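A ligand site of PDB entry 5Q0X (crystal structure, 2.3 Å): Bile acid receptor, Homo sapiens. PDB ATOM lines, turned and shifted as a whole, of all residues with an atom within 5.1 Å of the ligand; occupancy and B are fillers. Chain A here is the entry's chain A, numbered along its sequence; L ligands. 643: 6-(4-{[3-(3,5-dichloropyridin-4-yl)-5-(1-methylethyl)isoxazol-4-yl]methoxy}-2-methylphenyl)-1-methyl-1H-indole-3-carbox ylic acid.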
ATOM      1  N   ARG A  25      24.003  19.217  16.653  1.00  0.00           N
ATOM      2  CA  ARG A  25      22.965  18.494  15.936  1.00  0.00           C
ATOM      3  C   ARG A  25      22.476  19.299  14.744  1.00  0.00           C
ATOM      4  O   ARG A  25      22.392  20.531  14.803  1.00  0.00           O
ATOM      5  CB  ARG A  25      21.718  18.209  16.823  1.00  0.00           C
ATOM      6  CG  ARG A  25      21.936  17.421  18.114  1.00  0.00           C
ATOM      7  CD  ARG A  25      21.943  15.915  17.904  1.00  0.00           C
ATOM      8  NE  ARG A  25      22.100  15.203  19.183  1.00  0.00           N
ATOM      9  CZ  ARG A  25      23.266  14.994  19.799  1.00  0.00           C
ATOM     10  NH1 ARG A  25      24.396  15.447  19.267  1.00  0.00           N
ATOM     11  NH2 ARG A  25      23.301  14.342  20.944  1.00  0.00           N
ATOM     12  N   MET A  26      22.081  18.573  13.682  1.00  0.00           N
ATOM     13  CA  MET A  26      21.416  19.103  12.511  1.00  0.00           C
ATOM     14  C   MET A  26      19.942  18.716  12.754  1.00  0.00           C
ATOM     15  O   MET A  26      19.648  17.519  12.847  1.00  0.00           O
ATOM     16  CB  MET A  26      21.980  18.484  11.203  1.00  0.00           C
ATOM     17  CG  MET A  26      21.402  19.068   9.908  1.00  0.00           C
ATOM     18  SD  MET A  26      21.523  20.875   9.707  1.00  0.00           S
ATOM     19  CE  MET A  26      23.167  21.059   9.171  1.00  0.00           C
ATOM     20  N   THR A  31      17.197  17.876   7.921  1.00  0.00           N
ATOM     21  CA  THR A  31      17.648  16.611   7.318  1.00  0.00           C
ATOM     22  C   THR A  31      16.573  16.008   6.404  1.00  0.00           C
ATOM     23  O   THR A  31      16.920  15.454   5.361  1.00  0.00           O
ATOM     24  CB  THR A  31      18.166  15.602   8.356  1.00  0.00           C
ATOM     25  OG1 THR A  31      17.116  15.194   9.221  1.00  0.00           O
ATOM     26  CG2 THR A  31      19.324  16.114   9.162  1.00  0.00           C
ATOM     27  N   ILE A  34      16.630  17.464   2.853  1.00  0.00           N
ATOM     28  CA  ILE A  34      17.683  16.875   2.012  1.00  0.00           C
ATOM     29  C   ILE A  34      17.092  15.667   1.269  1.00  0.00           C
ATOM     30  O   ILE A  34      17.342  15.506   0.071  1.00  0.00           O
ATOM     31  CB  ILE A  34      18.952  16.491   2.830  1.00  0.00           C
ATOM     32  CG1 ILE A  34      19.580  17.716   3.560  1.00  0.00           C
ATOM     33  CG2 ILE A  34      20.007  15.775   1.949  1.00  0.00           C
ATOM     34  CD1 ILE A  34      20.533  17.353   4.783  1.00  0.00           C
ATOM     35  N   PHE A  45      20.402  25.201  -3.734  1.00  0.00           N
ATOM     36  CA  PHE A  45      21.087  26.350  -3.149  1.00  0.00           C
ATOM     37  C   PHE A  45      20.406  26.787  -1.842  1.00  0.00           C
ATOM     38  O   PHE A  45      21.108  27.120  -0.886  1.00  0.00           O
ATOM     39  CB  PHE A  45      21.190  27.520  -4.130  1.00  0.00           C
ATOM     40  CG  PHE A  45      22.130  28.596  -3.639  1.00  0.00           C
ATOM     41  CD1 PHE A  45      21.651  29.668  -2.886  1.00  0.00           C
ATOM     42  CD2 PHE A  45      23.490  28.515  -3.873  1.00  0.00           C
ATOM     43  CE1 PHE A  45      22.513  30.648  -2.395  1.00  0.00           C
ATOM     44  CE2 PHE A  45      24.357  29.512  -3.407  1.00  0.00           C
ATOM     45  CZ  PHE A  45      23.862  30.565  -2.670  1.00  0.00           C
ATOM     46  N   LEU A  48      21.365  24.385   0.967  1.00  0.00           N
ATOM     47  CA  LEU A  48      22.739  24.669   1.416  1.00  0.00           C
ATOM     48  C   LEU A  48      22.759  25.868   2.385  1.00  0.00           C
ATOM     49  O   LEU A  48      23.442  25.807   3.409  1.00  0.00           O
ATOM     50  CB  LEU A  48      23.735  24.899   0.254  1.00  0.00           C
ATOM     51  CG  LEU A  48      23.917  23.827  -0.842  1.00  0.00           C
ATOM     52  CD1 LEU A  48      25.161  24.091  -1.642  1.00  0.00           C
ATOM     53  CD2 LEU A  48      23.976  22.430  -0.283  1.00  0.00           C
ATOM     54  N   THR A  49      21.967  26.923   2.047  1.00  0.00           N
ATOM     55  CA  THR A  49      21.792  28.143   2.848  1.00  0.00           C
ATOM     56  C   THR A  49      21.228  27.824   4.246  1.00  0.00           C
ATOM     57  O   THR A  49      21.768  28.305   5.241  1.00  0.00           O
ATOM     58  CB  THR A  49      20.883  29.126   2.069  1.00  0.00           C
ATOM     59  OG1 THR A  49      21.537  29.474   0.852  1.00  0.00           O
ATOM     60  CG2 THR A  49      20.590  30.398   2.862  1.00  0.00           C
ATOM     61  N   MET A  51      21.223  24.884   5.872  1.00  0.00           N
ATOM     62  CA  MET A  51      22.218  24.076   6.579  1.00  0.00           C
ATOM     63  C   MET A  51      23.331  24.932   7.153  1.00  0.00           C
ATOM     64  O   MET A  51      23.746  24.721   8.285  1.00  0.00           O
ATOM     65  CB  MET A  51      22.812  22.983   5.671  1.00  0.00           C
ATOM     66  CG  MET A  51      21.822  21.877   5.320  1.00  0.00           C
ATOM     67  SD  MET A  51      22.558  20.516   4.381  1.00  0.00           S
ATOM     68  CE  MET A  51      22.922  21.316   2.905  1.00  0.00           C
ATOM     69  N   ALA A  52      23.807  25.922   6.366  1.00  0.00           N
ATOM     70  CA  ALA A  52      24.864  26.860   6.783  1.00  0.00           C
ATOM     71  C   ALA A  52      24.407  27.689   7.969  1.00  0.00           C
ATOM     72  O   ALA A  52      25.186  27.886   8.901  1.00  0.00           O
ATOM     73  CB  ALA A  52      25.238  27.767   5.621  1.00  0.00           C
ATOM     74  N   HIS A  55      24.331  25.477  11.060  1.00  0.00           N
ATOM     75  CA  HIS A  55      25.718  25.278  11.487  1.00  0.00           C
ATOM     76  C   HIS A  55      26.323  26.509  12.223  1.00  0.00           C
ATOM     77  O   HIS A  55      27.061  26.312  13.201  1.00  0.00           O
ATOM     78  CB  HIS A  55      26.636  24.818  10.339  1.00  0.00           C
ATOM     79  CG  HIS A  55      28.041  24.596  10.824  1.00  0.00           C
ATOM     80  ND1 HIS A  55      28.368  23.501  11.607  1.00  0.00           N
ATOM     81  CD2 HIS A  55      29.102  25.434  10.770  1.00  0.00           C
ATOM     82  CE1 HIS A  55      29.638  23.660  11.929  1.00  0.00           C
ATOM     83  NE2 HIS A  55      30.121  24.810  11.463  1.00  0.00           N
ATOM     84  N   VAL A  86      33.443  30.029   7.998  1.00  0.00           N
ATOM     85  CA  VAL A  86      33.626  29.251   6.756  1.00  0.00           C
ATOM     86  C   VAL A  86      34.530  28.040   7.035  1.00  0.00           C
ATOM     87  O   VAL A  86      34.173  26.919   6.672  1.00  0.00           O
ATOM     88  CB  VAL A  86      34.142  30.127   5.577  1.00  0.00           C
ATOM     89  CG1 VAL A  86      34.594  29.275   4.385  1.00  0.00           C
ATOM     90  CG2 VAL A  86      33.100  31.142   5.135  1.00  0.00           C
ATOM     91  N   MET A  89      32.784  25.386   9.054  1.00  0.00           N
ATOM     92  CA  MET A  89      31.742  24.785   8.234  1.00  0.00           C
ATOM     93  C   MET A  89      32.334  23.736   7.252  1.00  0.00           C
ATOM     94  O   MET A  89      31.729  22.674   7.082  1.00  0.00           O
ATOM     95  CB  MET A  89      30.976  25.860   7.499  1.00  0.00           C
ATOM     96  CG  MET A  89      29.576  25.449   7.164  1.00  0.00           C
ATOM     97  SD  MET A  89      28.717  26.841   6.428  1.00  0.00           S
ATOM     98  CE  MET A  89      28.463  27.870   7.883  1.00  0.00           C
ATOM     99  N   PHE A  90      33.515  24.026   6.660  1.00  0.00           N
ATOM    100  CA  PHE A  90      34.201  23.060   5.775  1.00  0.00           C
ATOM    101  C   PHE A  90      34.717  21.836   6.526  1.00  0.00           C
ATOM    102  O   PHE A  90      34.623  20.722   5.997  1.00  0.00           O
ATOM    103  CB  PHE A  90      35.332  23.720   4.974  1.00  0.00           C
ATOM    104  CG  PHE A  90      34.855  24.311   3.682  1.00  0.00           C
ATOM    105  CD1 PHE A  90      34.704  23.516   2.554  1.00  0.00           C
ATOM    106  CD2 PHE A  90      34.482  25.645   3.610  1.00  0.00           C
ATOM    107  CE1 PHE A  90      34.220  24.064   1.355  1.00  0.00           C
ATOM    108  CE2 PHE A  90      34.000  26.187   2.423  1.00  0.00           C
ATOM    109  CZ  PHE A  90      33.861  25.387   1.307  1.00  0.00           C
ATOM    110  N   ARG A  92      33.506  20.534   9.363  1.00  0.00           N
ATOM    111  CA  ARG A  92      32.341  19.768   9.755  1.00  0.00           C
ATOM    112  C   ARG A  92      31.750  19.031   8.565  1.00  0.00           C
ATOM    113  O   ARG A  92      31.342  17.881   8.713  1.00  0.00           O
ATOM    114  CB  ARG A  92      31.300  20.686  10.411  1.00  0.00           C
ATOM    115  CG  ARG A  92      30.076  19.970  11.016  1.00  0.00           C
ATOM    116  CD  ARG A  92      30.440  18.918  12.048  1.00  0.00           C
ATOM    117  NE  ARG A  92      29.242  18.249  12.559  1.00  0.00           N
ATOM    118  CZ  ARG A  92      29.234  17.348  13.528  1.00  0.00           C
ATOM    119  NH1 ARG A  92      30.378  16.983  14.100  1.00  0.00           N
ATOM    120  NH2 ARG A  92      28.104  16.807  13.927  1.00  0.00           N
ATOM    121  N   SER A  93      31.715  19.682   7.378  1.00  0.00           N
ATOM    122  CA  SER A  93      31.227  19.094   6.123  1.00  0.00           C
ATOM    123  C   SER A  93      32.082  17.893   5.799  1.00  0.00           C
ATOM    124  O   SER A  93      31.550  16.820   5.511  1.00  0.00           O
ATOM    125  CB  SER A  93      31.285  20.104   4.985  1.00  0.00           C
ATOM    126  OG  SER A  93      30.138  20.934   5.008  1.00  0.00           O
ATOM    127  N   ILE A  96      31.249  14.916   8.257  1.00  0.00           N
ATOM    128  CA  ILE A  96      29.975  14.233   8.015  1.00  0.00           C
ATOM    129  C   ILE A  96      30.037  13.398   6.721  1.00  0.00           C
ATOM    130  O   ILE A  96      29.443  12.309   6.681  1.00  0.00           O
ATOM    131  CB  ILE A  96      28.717  15.175   8.130  1.00  0.00           C
ATOM    132  CG1 ILE A  96      28.713  16.357   7.142  1.00  0.00           C
ATOM    133  CG2 ILE A  96      28.552  15.665   9.558  1.00  0.00           C
ATOM    134  CD1 ILE A  96      28.064  16.094   5.747  1.00  0.00           C
ATOM    135  N   LEU A 109      22.876  14.253  -0.606  1.00  0.00           N
ATOM    136  CA  LEU A 109      23.488  15.510  -0.185  1.00  0.00           C
ATOM    137  C   LEU A 109      24.576  15.918  -1.172  1.00  0.00           C
ATOM    138  O   LEU A 109      24.536  17.047  -1.673  1.00  0.00           O
ATOM    139  CB  LEU A 109      24.010  15.431   1.260  1.00  0.00           C
ATOM    140  CG  LEU A 109      24.711  16.675   1.822  1.00  0.00           C
ATOM    141  CD1 LEU A 109      23.753  17.858   1.940  1.00  0.00           C
ATOM    142  CD2 LEU A 109      25.311  16.370   3.182  1.00  0.00           C
ATOM    143  N   ILE A 113      24.769  19.406  -3.587  1.00  0.00           N
ATOM    144  CA  ILE A 113      25.942  20.296  -3.598  1.00  0.00           C
ATOM    145  C   ILE A 113      26.481  20.470  -5.033  1.00  0.00           C
ATOM    146  O   ILE A 113      26.710  21.607  -5.454  1.00  0.00           O
ATOM    147  CB  ILE A 113      27.037  19.804  -2.604  1.00  0.00           C
ATOM    148  CG1 ILE A 113      26.527  19.880  -1.138  1.00  0.00           C
ATOM    149  CG2 ILE A 113      28.368  20.586  -2.777  1.00  0.00           C
ATOM    150  CD1 ILE A 113      27.372  19.122  -0.087  1.00  0.00           C
ATOM    151  N   ILE A 118      26.649  26.159  -8.116  1.00  0.00           N
ATOM    152  CA  ILE A 118      27.974  26.551  -7.655  1.00  0.00           C
ATOM    153  C   ILE A 118      28.996  25.993  -8.629  1.00  0.00           C
ATOM    154  O   ILE A 118      28.940  24.797  -8.940  1.00  0.00           O
ATOM    155  CB  ILE A 118      28.246  26.168  -6.175  1.00  0.00           C
ATOM    156  CG1 ILE A 118      27.313  26.939  -5.210  1.00  0.00           C
ATOM    157  CG2 ILE A 118      29.726  26.397  -5.801  1.00  0.00           C
ATOM    158  CD1 ILE A 118      27.379  26.482  -3.679  1.00  0.00           C
ATOM    159  N   TYR A 122      34.940  25.967  -7.328  1.00  0.00           N
ATOM    160  CA  TYR A 122      34.724  25.902  -5.886  1.00  0.00           C
ATOM    161  C   TYR A 122      34.486  24.447  -5.448  1.00  0.00           C
ATOM    162  O   TYR A 122      35.119  23.979  -4.500  1.00  0.00           O
ATOM    163  CB  TYR A 122      33.543  26.817  -5.504  1.00  0.00           C
ATOM    164  CG  TYR A 122      33.333  27.125  -4.031  1.00  0.00           C
ATOM    165  CD1 TYR A 122      34.282  26.755  -3.074  1.00  0.00           C
ATOM    166  CD2 TYR A 122      32.220  27.825  -3.602  1.00  0.00           C
ATOM    167  CE1 TYR A 122      34.087  27.034  -1.728  1.00  0.00           C
ATOM    168  CE2 TYR A 122      32.015  28.104  -2.246  1.00  0.00           C
ATOM    169  CZ  TYR A 122      32.948  27.712  -1.316  1.00  0.00           C
ATOM    170  OH  TYR A 122      32.752  27.996   0.009  1.00  0.00           O
ATOM    171  N   MET A 126      36.845  21.614  -2.865  1.00  0.00           N
ATOM    172  CA  MET A 126      35.933  21.215  -1.781  1.00  0.00           C
ATOM    173  C   MET A 126      35.924  19.686  -1.614  1.00  0.00           C
ATOM    174  O   MET A 126      36.198  19.182  -0.517  1.00  0.00           O
ATOM    175  CB  MET A 126      34.522  21.749  -2.127  1.00  0.00           C
ATOM    176  CG  MET A 126      33.442  21.388  -1.131  1.00  0.00           C
ATOM    177  SD  MET A 126      31.803  21.904  -1.720  1.00  0.00           S
ATOM    178  CE  MET A 126      31.983  23.699  -1.740  1.00  0.00           C
ATOM    179  N   TYR A 130      37.640  17.048   1.275  1.00  0.00           N
ATOM    180  CA  TYR A 130      36.921  15.949   1.934  1.00  0.00           C
ATOM    181  C   TYR A 130      37.682  14.651   1.785  1.00  0.00           C
ATOM    182  O   TYR A 130      37.681  13.836   2.712  1.00  0.00           O
ATOM    183  CB  TYR A 130      35.538  15.722   1.305  1.00  0.00           C
ATOM    184  CG  TYR A 130      34.534  16.840   1.427  1.00  0.00           C
ATOM    185  CD1 TYR A 130      34.762  17.943   2.264  1.00  0.00           C
ATOM    186  CD2 TYR A 130      33.336  16.805   0.727  1.00  0.00           C
ATOM    187  CE1 TYR A 130      33.841  18.981   2.358  1.00  0.00           C
ATOM    188  CE2 TYR A 130      32.415  17.840   0.811  1.00  0.00           C
ATOM    189  CZ  TYR A 130      32.662  18.913   1.636  1.00  0.00           C
ATOM    190  OH  TYR A 130      31.713  19.898   1.721  1.00  0.00           O
ATOM    191  N   HIS A 208      35.061  31.086  -0.962  1.00  0.00           N
ATOM    192  CA  HIS A 208      33.731  31.395  -0.454  1.00  0.00           C
ATOM    193  C   HIS A 208      33.323  32.844  -0.742  1.00  0.00           C
ATOM    194  O   HIS A 208      32.164  33.091  -1.058  1.00  0.00           O
ATOM    195  CB  HIS A 208      33.609  31.095   1.050  1.00  0.00           C
ATOM    196  CG  HIS A 208      32.196  31.087   1.531  1.00  0.00           C
ATOM    197  ND1 HIS A 208      31.410  29.940   1.468  1.00  0.00           N
ATOM    198  CD2 HIS A 208      31.464  32.080   2.078  1.00  0.00           C
ATOM    199  CE1 HIS A 208      30.237  30.281   1.974  1.00  0.00           C
ATOM    200  NE2 HIS A 208      30.212  31.556   2.344  1.00  0.00           N
ATOM    201  N   MET A 211      32.316  33.221  -4.345  1.00  0.00           N
ATOM    202  CA  MET A 211      31.002  32.613  -4.545  1.00  0.00           C
ATOM    203  C   MET A 211      29.894  33.607  -4.138  1.00  0.00           C
ATOM    204  O   MET A 211      28.940  33.781  -4.901  1.00  0.00           O
ATOM    205  CB  MET A 211      30.885  31.281  -3.761  1.00  0.00           C
ATOM    206  CG  MET A 211      29.578  30.526  -3.996  1.00  0.00           C
ATOM    207  SD  MET A 211      28.440  30.585  -2.561  1.00  0.00           S
ATOM    208  CE  MET A 211      27.214  31.656  -3.169  1.00  0.00           C
ATOM    209  N   PHE A 222      19.922  34.791   1.113  1.00  0.00           N
ATOM    210  CA  PHE A 222      20.537  34.050   2.221  1.00  0.00           C
ATOM    211  C   PHE A 222      19.618  34.086   3.465  1.00  0.00           C
ATOM    212  O   PHE A 222      18.398  33.994   3.345  1.00  0.00           O
ATOM    213  CB  PHE A 222      21.974  34.554   2.545  1.00  0.00           C
ATOM    214  CG  PHE A 222      22.920  34.545   1.379  1.00  0.00           C
ATOM    215  CD1 PHE A 222      23.628  33.388   1.048  1.00  0.00           C
ATOM    216  CD2 PHE A 222      23.110  35.676   0.607  1.00  0.00           C
ATOM    217  CE1 PHE A 222      24.484  33.371  -0.058  1.00  0.00           C
ATOM    218  CE2 PHE A 222      23.985  35.666  -0.490  1.00  0.00           C
ATOM    219  CZ  PHE A 222      24.664  34.505  -0.810  1.00  0.00           C
ATOM    220  N   LEU A 226      23.744  34.617   8.184  1.00  0.00           N
ATOM    221  CA  LEU A 226      24.800  34.477   7.179  1.00  0.00           C
ATOM    222  C   LEU A 226      25.227  35.828   6.599  1.00  0.00           C
ATOM    223  O   LEU A 226      26.418  36.037   6.378  1.00  0.00           O
ATOM    224  CB  LEU A 226      24.346  33.534   6.045  1.00  0.00           C
ATOM    225  CG  LEU A 226      24.052  32.089   6.417  1.00  0.00           C
ATOM    226  CD1 LEU A 226      23.660  31.298   5.186  1.00  0.00           C
ATOM    227  CD2 LEU A 226      25.235  31.432   7.136  1.00  0.00           C
ATOM    228  N   TRP A 230      29.215  37.114   7.130  1.00  0.00           N
ATOM    229  CA  TRP A 230      29.957  37.240   5.870  1.00  0.00           C
ATOM    230  C   TRP A 230      29.877  38.626   5.209  1.00  0.00           C
ATOM    231  O   TRP A 230      30.359  38.772   4.088  1.00  0.00           O
ATOM    232  CB  TRP A 230      29.533  36.123   4.895  1.00  0.00           C
ATOM    233  CG  TRP A 230      29.845  34.744   5.388  1.00  0.00           C
ATOM    234  CD1 TRP A 230      30.904  34.367   6.165  1.00  0.00           C
ATOM    235  CD2 TRP A 230      29.121  33.533   5.095  1.00  0.00           C
ATOM    236  NE1 TRP A 230      30.841  33.018   6.419  1.00  0.00           N
ATOM    237  CE2 TRP A 230      29.788  32.471   5.739  1.00  0.00           C
ATOM    238  CE3 TRP A 230      27.980  33.236   4.318  1.00  0.00           C
ATOM    239  CZ2 TRP A 230      29.338  31.144   5.662  1.00  0.00           C
ATOM    240  CZ3 TRP A 230      27.536  31.924   4.248  1.00  0.00           C
ATOM    241  CH2 TRP A 230      28.204  30.902   4.923  1.00  0.00           C
HETATM  242  C4  643 L   1      26.668  19.879   9.434  1.00  0.00           C
HETATM  243  C5  643 L   1      25.417  17.655  10.097  1.00  0.00           C
HETATM  244  C6  643 L   1      25.866  18.740   9.254  1.00  0.00           C
HETATM  245  C7  643 L   1      25.304  18.514   7.988  1.00  0.00           C
HETATM  246  C10 643 L   1      23.814  16.761   6.944  1.00  0.00           C
HETATM  247  C15 643 L   1      26.347  22.801   6.160  1.00  0.00           C
HETATM  248  C17 643 L   1      26.893  21.006   4.620  1.00  0.00           C
HETATM  249  C21 643 L   1      29.745  24.907   1.621  1.00  0.00           C
HETATM  250  C22 643 L   1      29.718  23.617   1.088  1.00  0.00           C
HETATM  251  C26 643 L   1      30.469  25.061   2.809  1.00  0.00           C
HETATM  252  C28 643 L   1      27.490  26.225   1.787  1.00  0.00           C
HETATM  253  C1  643 L   1      26.889  20.746   8.359  1.00  0.00           C
HETATM  254  C2  643 L   1      26.343  20.501   7.088  1.00  0.00           C
HETATM  255  C3  643 L   1      25.528  19.374   6.925  1.00  0.00           C
HETATM  256  N8  643 L   1      24.555  17.355   8.042  1.00  0.00           N
HETATM  257  C9  643 L   1      24.635  16.853   9.307  1.00  0.00           C
HETATM  258  C11 643 L   1      25.705  17.404  11.534  1.00  0.00           C
HETATM  259  O12 643 L   1      26.425  18.151  12.180  1.00  0.00           O
HETATM  260  O13 643 L   1      25.148  16.342  12.046  1.00  0.00           O
HETATM  261  C14 643 L   1      26.492  23.726   5.139  1.00  0.00           C
HETATM  262  C16 643 L   1      26.544  21.436   5.922  1.00  0.00           C
HETATM  263  C18 643 L   1      27.042  21.955   3.604  1.00  0.00           C
HETATM  264  C19 643 L   1      26.849  23.307   3.866  1.00  0.00           C
HETATM  265  O20 643 L   1      27.018  24.140   2.796  1.00  0.00           O
HETATM  266  C23 643 L   1      30.251  22.558   1.798  1.00  0.00           C
HETATM  267  N24 643 L   1      31.114  22.798   2.805  1.00  0.00           N
HETATM  268  C25 643 L   1      31.059  23.976   3.446  1.00  0.00           C
HETATM  269  C27 643 L   1      28.762  25.932   1.200  1.00  0.00           C
HETATM  270  C29 643 L   1      27.022  27.230   1.051  1.00  0.00           C
HETATM  271  O30 643 L   1      27.900  27.576   0.082  1.00  0.00           O
HETATM  272  N31 643 L   1      29.026  26.723   0.197  1.00  0.00           N
HETATM  273 CL32 643 L   1      28.626  23.242  -0.204  1.00  0.00          CL
HETATM  274  C33 643 L   1      25.723  28.048   1.102  1.00  0.00           C
HETATM  275  C34 643 L   1      25.934  29.364   1.833  1.00  0.00           C
HETATM  276  C35 643 L   1      25.107  28.213  -0.285  1.00  0.00           C
HETATM  277  C36 643 L   1      26.859  25.549   2.952  1.00  0.00           C
HETATM  278 CL37 643 L   1      30.830  26.654   3.383  1.00  0.00          CL
HETATM  279  C38 643 L   1      27.130  19.553   4.252  1.00  0.00           C
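NH2 of Arg 92 is in salt-bridge range of O12 of the ligand (2.8 Å).
The side-chain hydroxyl (OH) of Tyr 130 sits close to a nitrogen (N24) of the ligand (3.2 Å).
A nitrogen (N24) of the ligand is in hydrogen-bond range of the side-chain hydroxyl of Ser 93 (3.0 Å).
The side-chain hydroxyl (OG) of Ser 93 lies within hydrogen-bond range of the backbone carbonyl oxygen (O) of Met 89, 3.1 Å away.
O of Phe 45 sits at hydrogen-bond distance from OG1 of Thr 49 (3.0 Å).
ND1 of His 208 sits at hydrogen-bond distance from OH of Tyr 122, at 2.8 Å.
Met 26 touches the ligand.
CD1 of Ile 34 touches C10 of the ligand, 3.97 Å away.
Phe 45 touches the ligand.
Leu 48 touches the ligand (O to C36, 3.5 Å).
Thr 49 touches the ligand.
Met 51 touches the ligand.
Ala 52 touches the ligand.
Met 89 touches the ligand.
CE2 of Phe 90 touches CL37 of the ligand, 3.3 Å away.
Ile 96 touches the ligand.
Leu 109 touches the ligand (CD2 to C38, 3.8 Å).
Ile 113 touches the ligand (CG2 to CL32, 3.7 Å).
Ile 118 touches the ligand (CD1 to O30, 3.95 Å).
Tyr 122 touches the ligand (OH to N31, 3.9 Å).
Met 126 touches the ligand.
His 208 touches the ligand (ND1 to CL37, 3.8 Å).
CZ3 of Trp 230 touches C34 of the ligand, 3.9 Å away.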
